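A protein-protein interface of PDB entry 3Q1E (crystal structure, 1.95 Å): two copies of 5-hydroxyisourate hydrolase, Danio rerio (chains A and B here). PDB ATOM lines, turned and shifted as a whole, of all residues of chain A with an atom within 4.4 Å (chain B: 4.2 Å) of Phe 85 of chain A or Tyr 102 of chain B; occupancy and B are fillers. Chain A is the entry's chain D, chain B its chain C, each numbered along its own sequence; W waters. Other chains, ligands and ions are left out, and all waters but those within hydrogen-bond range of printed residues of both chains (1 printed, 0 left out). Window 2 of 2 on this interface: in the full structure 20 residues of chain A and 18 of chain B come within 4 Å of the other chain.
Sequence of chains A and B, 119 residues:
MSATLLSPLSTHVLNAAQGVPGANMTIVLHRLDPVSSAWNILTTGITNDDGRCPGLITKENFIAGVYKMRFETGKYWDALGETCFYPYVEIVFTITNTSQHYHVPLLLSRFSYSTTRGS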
ATOM      1  N   CYS A  84       6.556  11.214  23.838  1.00  0.00           N
ATOM      2  CA  CYS A  84       7.942  11.718  23.932  1.00  0.00           C
ATOM      3  C   CYS A  84       8.819  10.838  23.021  1.00  0.00           C
ATOM      4  O   CYS A  84       8.532   9.673  22.859  1.00  0.00           O
ATOM      5  CB  CYS A  84       8.426  11.661  25.388  1.00  0.00           C
ATOM      6  SG  CYS A  84      10.064  12.405  25.698  1.00  0.00           S
ATOM      7  N   PHE A  85       9.798  11.424  22.341  1.00  0.00           N
ATOM      8  CA  PHE A  85      10.787  10.654  21.570  1.00  0.00           C
ATOM      9  C   PHE A  85      11.597   9.636  22.446  1.00  0.00           C
ATOM     10  O   PHE A  85      11.987   8.553  21.996  1.00  0.00           O
ATOM     11  CB  PHE A  85      11.782  11.613  20.854  1.00  0.00           C
ATOM     12  CG  PHE A  85      12.680  10.923  19.856  1.00  0.00           C
ATOM     13  CD1 PHE A  85      12.145  10.023  18.921  1.00  0.00           C
ATOM     14  CD2 PHE A  85      14.089  11.173  19.840  1.00  0.00           C
ATOM     15  CE1 PHE A  85      12.991   9.346  18.006  1.00  0.00           C
ATOM     16  CE2 PHE A  85      14.905  10.525  18.923  1.00  0.00           C
ATOM     17  CZ  PHE A  85      14.395   9.611  18.014  1.00  0.00           C
ATOM     18  N   TYR A  86      11.804   9.999  23.698  1.00  0.00           N
ATOM     19  CA  TYR A  86      12.681   9.271  24.608  1.00  0.00           C
ATOM     20  C   TYR A  86      11.797   8.682  25.651  1.00  0.00           C
ATOM     21  O   TYR A  86      11.161   9.430  26.366  1.00  0.00           O
ATOM     22  CB  TYR A  86      13.624  10.278  25.287  1.00  0.00           C
ATOM     23  CG  TYR A  86      14.226  11.228  24.310  1.00  0.00           C
ATOM     24  CD1 TYR A  86      15.392  10.865  23.561  1.00  0.00           C
ATOM     25  CD2 TYR A  86      13.686  12.509  24.129  1.00  0.00           C
ATOM     26  CE1 TYR A  86      15.935  11.706  22.620  1.00  0.00           C
ATOM     27  CE2 TYR A  86      14.290  13.420  23.202  1.00  0.00           C
ATOM     28  CZ  TYR A  86      15.406  12.986  22.483  1.00  0.00           C
ATOM     29  OH  TYR A  86      15.955  13.793  21.585  1.00  0.00           O
ATOM     30  N   PRO A  87      11.757   7.324  25.779  1.00  0.00           N
ATOM     31  CA  PRO A  87      10.975   6.742  26.906  1.00  0.00           C
ATOM     32  C   PRO A  87      11.447   7.110  28.327  1.00  0.00           C
ATOM     33  O   PRO A  87      10.639   7.232  29.288  1.00  0.00           O
ATOM     34  CB  PRO A  87      11.117   5.215  26.703  1.00  0.00           C
ATOM     35  CG  PRO A  87      11.997   5.008  25.513  1.00  0.00           C
ATOM     36  CD  PRO A  87      12.301   6.321  24.859  1.00  0.00           C
ATOM     37  N   ARG A 110       9.251  17.428  24.028  1.00  0.00           N
ATOM     38  CA  ARG A 110       8.930  16.074  23.546  1.00  0.00           C
ATOM     39  C   ARG A 110      10.005  15.483  22.660  1.00  0.00           C
ATOM     40  O   ARG A 110      10.046  14.276  22.526  1.00  0.00           O
ATOM     41  CB  ARG A 110       7.616  16.048  22.790  1.00  0.00           C
ATOM     42  CG  ARG A 110       6.430  16.470  23.590  1.00  0.00           C
ATOM     43  CD  ARG A 110       5.193  15.844  22.919  1.00  0.00           C
ATOM     44  NE  ARG A 110       4.825  16.544  21.721  1.00  0.00           N
ATOM     45  CZ  ARG A 110       4.281  16.012  20.627  1.00  0.00           C
ATOM     46  NH1 ARG A 110       4.100  14.695  20.505  1.00  0.00           N
ATOM     47  NH2 ARG A 110       3.954  16.831  19.627  1.00  0.00           N
ATOM     48  N   PHE A 111      10.890  16.323  22.104  1.00  0.00           N
ATOM     49  CA  PHE A 111      11.859  15.877  21.097  1.00  0.00           C
ATOM     50  C   PHE A 111      13.312  16.382  21.278  1.00  0.00           C
ATOM     51  O   PHE A 111      14.093  16.271  20.351  1.00  0.00           O
ATOM     52  CB  PHE A 111      11.410  16.252  19.674  1.00  0.00           C
ATOM     53  CG  PHE A 111      10.112  15.636  19.271  1.00  0.00           C
ATOM     54  CD1 PHE A 111      10.070  14.324  18.800  1.00  0.00           C
ATOM     55  CD2 PHE A 111       8.925  16.344  19.425  1.00  0.00           C
ATOM     56  CE1 PHE A 111       8.862  13.734  18.466  1.00  0.00           C
ATOM     57  CE2 PHE A 111       7.685  15.777  19.084  1.00  0.00           C
ATOM     58  CZ  PHE A 111       7.640  14.465  18.602  1.00  0.00           C
ATOM     59  N   PRO B   8      19.176   4.784   7.383  1.00  0.00           N
ATOM     60  CA  PRO B   8      18.031   5.581   7.853  1.00  0.00           C
ATOM     61  C   PRO B   8      18.200   6.171   9.288  1.00  0.00           C
ATOM     62  O   PRO B   8      17.329   6.910   9.774  1.00  0.00           O
ATOM     63  CB  PRO B   8      16.867   4.568   7.816  1.00  0.00           C
ATOM     64  CG  PRO B   8      17.531   3.254   8.101  1.00  0.00           C
ATOM     65  CD  PRO B   8      18.866   3.337   7.366  1.00  0.00           C
ATOM     66  N   LEU B   9      19.316   5.860   9.944  1.00  0.00           N
ATOM     67  CA  LEU B   9      19.658   6.405  11.276  1.00  0.00           C
ATOM     68  C   LEU B   9      21.015   7.109  11.176  1.00  0.00           C
ATOM     69  O   LEU B   9      22.005   6.490  10.815  1.00  0.00           O
ATOM     70  CB  LEU B   9      19.700   5.269  12.319  1.00  0.00           C
ATOM     71  CG  LEU B   9      20.088   5.587  13.766  1.00  0.00           C
ATOM     72  CD1 LEU B   9      19.274   6.748  14.396  1.00  0.00           C
ATOM     73  CD2 LEU B   9      20.002   4.322  14.588  1.00  0.00           C
ATOM     74  N   SER B  10      21.072   8.390  11.481  1.00  0.00           N
ATOM     75  CA  SER B  10      22.373   9.062  11.451  1.00  0.00           C
ATOM     76  C   SER B  10      22.668   9.868  12.729  1.00  0.00           C
ATOM     77  O   SER B  10      21.783  10.091  13.534  1.00  0.00           O
ATOM     78  CB  SER B  10      22.465   9.992  10.223  1.00  0.00           C
ATOM     79  OG  SER B  10      21.481  10.996  10.297  1.00  0.00           O
ATOM     80  N   PHE B  62      16.316  -2.025  10.120  1.00  0.00           N
ATOM     81  CA  PHE B  62      15.841  -0.881  10.883  1.00  0.00           C
ATOM     82  C   PHE B  62      14.346  -1.054  11.155  1.00  0.00           C
ATOM     83  O   PHE B  62      13.476  -0.437  10.515  1.00  0.00           O
ATOM     84  CB  PHE B  62      16.183   0.416  10.124  1.00  0.00           C
ATOM     85  CG  PHE B  62      15.797   1.689  10.833  1.00  0.00           C
ATOM     86  CD1 PHE B  62      16.347   2.016  12.084  1.00  0.00           C
ATOM     87  CD2 PHE B  62      14.939   2.605  10.211  1.00  0.00           C
ATOM     88  CE1 PHE B  62      16.012   3.218  12.735  1.00  0.00           C
ATOM     89  CE2 PHE B  62      14.592   3.824  10.841  1.00  0.00           C
ATOM     90  CZ  PHE B  62      15.135   4.131  12.101  1.00  0.00           C
ATOM     91  N   PHE B  93      15.543   6.032  22.644  1.00  0.00           N
ATOM     92  CA  PHE B  93      14.529   6.639  21.861  1.00  0.00           C
ATOM     93  C   PHE B  93      13.694   5.606  21.177  1.00  0.00           C
ATOM     94  O   PHE B  93      14.171   4.515  20.880  1.00  0.00           O
ATOM     95  CB  PHE B  93      15.086   7.606  20.819  1.00  0.00           C
ATOM     96  CG  PHE B  93      16.166   7.008  19.912  1.00  0.00           C
ATOM     97  CD1 PHE B  93      17.527   7.064  20.296  1.00  0.00           C
ATOM     98  CD2 PHE B  93      15.837   6.422  18.705  1.00  0.00           C
ATOM     99  CE1 PHE B  93      18.556   6.528  19.478  1.00  0.00           C
ATOM    100  CE2 PHE B  93      16.852   5.905  17.855  1.00  0.00           C
ATOM    101  CZ  PHE B  93      18.242   5.965  18.270  1.00  0.00           C
ATOM    102  N   THR B  94      12.467   6.006  20.866  1.00  0.00           N
ATOM    103  CA  THR B  94      11.459   5.110  20.288  1.00  0.00           C
ATOM    104  C   THR B  94      11.265   5.385  18.782  1.00  0.00           C
ATOM    105  O   THR B  94      11.016   6.533  18.388  1.00  0.00           O
ATOM    106  CB  THR B  94      10.158   5.305  21.040  1.00  0.00           C
ATOM    107  OG1 THR B  94      10.434   5.070  22.419  1.00  0.00           O
ATOM    108  CG2 THR B  94       9.027   4.288  20.599  1.00  0.00           C
ATOM    109  N   ILE B  95      11.431   4.329  17.972  1.00  0.00           N
ATOM    110  CA  ILE B  95      11.204   4.335  16.551  1.00  0.00           C
ATOM    111  C   ILE B  95       9.866   3.647  16.279  1.00  0.00           C
ATOM    112  O   ILE B  95       9.698   2.410  16.394  1.00  0.00           O
ATOM    113  CB  ILE B  95      12.325   3.618  15.775  1.00  0.00           C
ATOM    114  CG1 ILE B  95      13.674   4.353  15.993  1.00  0.00           C
ATOM    115  CG2 ILE B  95      11.941   3.458  14.275  1.00  0.00           C
ATOM    116  CD1 ILE B  95      13.639   5.818  15.627  1.00  0.00           C
ATOM    117  N   ASN B  97       7.867   4.996  13.392  1.00  0.00           N
ATOM    118  CA  ASN B  97       7.678   5.091  11.912  1.00  0.00           C
ATOM    119  C   ASN B  97       8.980   4.860  11.115  1.00  0.00           C
ATOM    120  O   ASN B  97       9.858   5.725  11.020  1.00  0.00           O
ATOM    121  CB  ASN B  97       6.941   6.374  11.496  1.00  0.00           C
ATOM    122  CG  ASN B  97       6.695   6.460   9.999  1.00  0.00           C
ATOM    123  OD1 ASN B  97       7.264   5.702   9.195  1.00  0.00           O
ATOM    124  ND2 ASN B  97       5.835   7.399   9.606  1.00  0.00           N
ATOM    125  N   GLN B 100      10.651   6.969   7.866  1.00  0.00           N
ATOM    126  CA  GLN B 100      11.285   8.245   8.135  1.00  0.00           C
ATOM    127  C   GLN B 100      12.771   8.077   8.425  1.00  0.00           C
ATOM    128  O   GLN B 100      13.219   7.012   8.885  1.00  0.00           O
ATOM    129  CB  GLN B 100      10.669   8.884   9.359  1.00  0.00           C
ATOM    130  CG  GLN B 100       9.722  10.050   9.131  1.00  0.00           C
ATOM    131  CD  GLN B 100       8.659  10.060  10.198  1.00  0.00           C
ATOM    132  OE1 GLN B 100       7.549   9.555   9.991  1.00  0.00           O
ATOM    133  NE2 GLN B 100       9.005  10.558  11.369  1.00  0.00           N
ATOM    134  N   HIS B 101      13.511   9.152   8.154  1.00  0.00           N
ATOM    135  CA  HIS B 101      14.876   9.316   8.610  1.00  0.00           C
ATOM    136  C   HIS B 101      14.976   9.908  10.024  1.00  0.00           C
ATOM    137  O   HIS B 101      14.262  10.847  10.364  1.00  0.00           O
ATOM    138  CB  HIS B 101      15.642  10.246   7.667  1.00  0.00           C
ATOM    139  CG  HIS B 101      17.125  10.151   7.847  1.00  0.00           C
ATOM    140  ND1 HIS B 101      17.827  10.981   8.700  1.00  0.00           N
ATOM    141  CD2 HIS B 101      18.028   9.283   7.341  1.00  0.00           C
ATOM    142  CE1 HIS B 101      19.105  10.651   8.676  1.00  0.00           C
ATOM    143  NE2 HIS B 101      19.247   9.615   7.870  1.00  0.00           N
ATOM    144  N   TYR B 102      15.928   9.403  10.808  1.00  0.00           N
ATOM    145  CA  TYR B 102      16.116   9.836  12.212  1.00  0.00           C
ATOM    146  C   TYR B 102      17.548  10.238  12.386  1.00  0.00           C
ATOM    147  O   TYR B 102      18.435   9.442  12.198  1.00  0.00           O
ATOM    148  CB  TYR B 102      15.760   8.705  13.175  1.00  0.00           C
ATOM    149  CG  TYR B 102      14.308   8.360  13.170  1.00  0.00           C
ATOM    150  CD1 TYR B 102      13.422   8.970  14.063  1.00  0.00           C
ATOM    151  CD2 TYR B 102      13.795   7.467  12.222  1.00  0.00           C
ATOM    152  CE1 TYR B 102      12.067   8.657  14.044  1.00  0.00           C
ATOM    153  CE2 TYR B 102      12.447   7.150  12.184  1.00  0.00           C
ATOM    154  CZ  TYR B 102      11.584   7.743  13.107  1.00  0.00           C
ATOM    155  OH  TYR B 102      10.243   7.411  13.082  1.00  0.00           O
ATOM    156  N   HIS B 103      17.771  11.508  12.685  1.00  0.00           N
ATOM    157  CA  HIS B 103      19.088  12.034  12.968  1.00  0.00           C
ATOM    158  C   HIS B 103      19.137  12.296  14.460  1.00  0.00           C
ATOM    159  O   HIS B 103      18.376  13.148  14.941  1.00  0.00           O
ATOM    160  CB  HIS B 103      19.249  13.383  12.267  1.00  0.00           C
ATOM    161  CG  HIS B 103      20.655  13.895  12.255  1.00  0.00           C
ATOM    162  ND1 HIS B 103      21.015  15.116  12.804  1.00  0.00           N
ATOM    163  CD2 HIS B 103      21.791  13.348  11.775  1.00  0.00           C
ATOM    164  CE1 HIS B 103      22.313  15.298  12.648  1.00  0.00           C
ATOM    165  NE2 HIS B 103      22.805  14.241  12.015  1.00  0.00           N
ATOM    166  N   VAL B 104      20.068  11.662  15.167  1.00  0.00           N
ATOM    167  CA  VAL B 104      20.165  11.775  16.623  1.00  0.00           C
ATOM    168  C   VAL B 104      21.543  12.360  16.976  1.00  0.00           C
ATOM    169  O   VAL B 104      22.481  11.610  17.161  1.00  0.00           O
ATOM    170  CB  VAL B 104      19.993  10.414  17.285  1.00  0.00           C
ATOM    171  CG1 VAL B 104      19.990  10.508  18.846  1.00  0.00           C
ATOM    172  CG2 VAL B 104      18.672   9.807  16.851  1.00  0.00           C
ATOM    173  N   ARG B 117      15.827  15.388  18.128  1.00  0.00           N
ATOM    174  CA  ARG B 117      15.535  14.485  17.037  1.00  0.00           C
ATOM    175  C   ARG B 117      15.474  15.340  15.764  1.00  0.00           C
ATOM    176  O   ARG B 117      14.873  16.428  15.750  1.00  0.00           O
ATOM    177  CB  ARG B 117      14.251  13.689  17.316  1.00  0.00           C
ATOM    178  CG  ARG B 117      13.628  12.867  16.148  1.00  0.00           C
ATOM    179  CD  ARG B 117      12.642  13.788  15.425  1.00  0.00           C
ATOM    180  NE  ARG B 117      11.536  13.127  14.774  1.00  0.00           N
ATOM    181  CZ  ARG B 117      11.612  12.532  13.586  1.00  0.00           C
ATOM    182  NH1 ARG B 117      12.755  12.468  12.915  1.00  0.00           N
ATOM    183  NH2 ARG B 117      10.538  11.969  13.081  1.00  0.00           N
ATOM    184  N   GLY B 118      16.155  14.862  14.729  1.00  0.00           N
ATOM    185  CA  GLY B 118      16.190  15.521  13.417  1.00  0.00           C
ATOM    186  C   GLY B 118      15.655  14.625  12.314  1.00  0.00           C
ATOM    187  O   GLY B 118      15.221  13.459  12.523  1.00  0.00           O
HETATM  188  O   HOH W   1       9.347   6.983  23.704  1.00  0.00           O
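Water W1 bridges OG1 of Thr 94 of chain B (2.5 Å) and O of Cys 84 of chain A (2.9 Å).
No position is printed for both chains.
Of the 8 pairs that touch across the chains among the printed residues, none has its exchanged pair printed and touching as well.
Among the printed residues, merely in contact across the chains: Phe 85 of chain A with Phe 93 of chain B, Phe 85 of chain A with Tyr 102 of chain B, Phe 85 of chain A with Arg 117 of chain B, Tyr 86 of chain A with Arg 117 of chain B, Pro 87 of chain A with Phe 93 of chain B and Pro 87 of chain A with Thr 94 of chain B.
N of Thr 94 of chain B is in hydrogen-bond range of O of Phe 85 of chain A.
O of Phe 111 of chain A sits at hydrogen-bond distance from N of Arg 117 of chain B (3.0 Å).
Printed residues of chain B that touch a printed residue of chain A: Phe 93, Thr 94, Tyr 102 and Arg 117.
Hydrophobic or aromatic side chains of chain B that line the printed part of chain A: Phe 93 and Tyr 102.
Printed residues of chain A that touch a printed residue of chain B: Phe 85, Tyr 86, Pro 87 and Phe 111.
Among the printed residues, 8 pairs touch across the chains.
Among the printed residues, no Asp or Glu carboxylate lies within 4 Å of a Lys or Arg side-chain nitrogen of the other chain.
The side-chain sulfur (SG) of Cys 84 of chain A is in hydrogen-bond range of the backbone carbonyl oxygen (O) of Tyr 86 of chain A (3.2 Å).
The backbone NH (N) of Tyr 102 of chain B sits at hydrogen-bond distance from the backbone carbonyl oxygen (O) of Pro 8 of chain B.
The backbone NH of Ser 10 of chain B is in hydrogen-bond range of the backbone carbonyl oxygen of Tyr 102 of chain B (2.9 Å).
The backbone NH (N) of Phe 85 of chain A sits at hydrogen-bond distance from the backbone carbonyl oxygen (O) of Arg 110 of chain A.
The backbone carbonyl oxygen (O) of Asn 97 of chain B lies within hydrogen-bond range of the side-chain hydroxyl (OH) of Tyr 102 of chain B (2.7 Å).
The side-chain amide nitrogen of Gln 100 of chain B sits close to the guanidinium group of Arg 117 of chain B (2.7 Å).
Printed residues of chain B within 4 Å of Phe 85 of chain A: Phe 93, Thr 94, Tyr 102 and Arg 117.
Printed residues of chain A within 4 Å of Thr 94 of chain B: Phe 85 and Pro 87.
Of the printed residues of chain B, Phe 111 of chain A touches Arg 117.
Of the printed residues of chain B, Tyr 86 of chain A touches Arg 117 (3.8 Å).
Of the printed residues of chain A, Arg 117 of chain B touches Phe 85, Tyr 86 and Phe 111.
The nearest printed residue of chain B that does not touch Phe 85 of chain A is Ile 95 of chain B (4.3 Å).
The nearest printed residue of chain B that does not touch Pro 87 of chain A is Ile 95 of chain B (7.2 Å).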
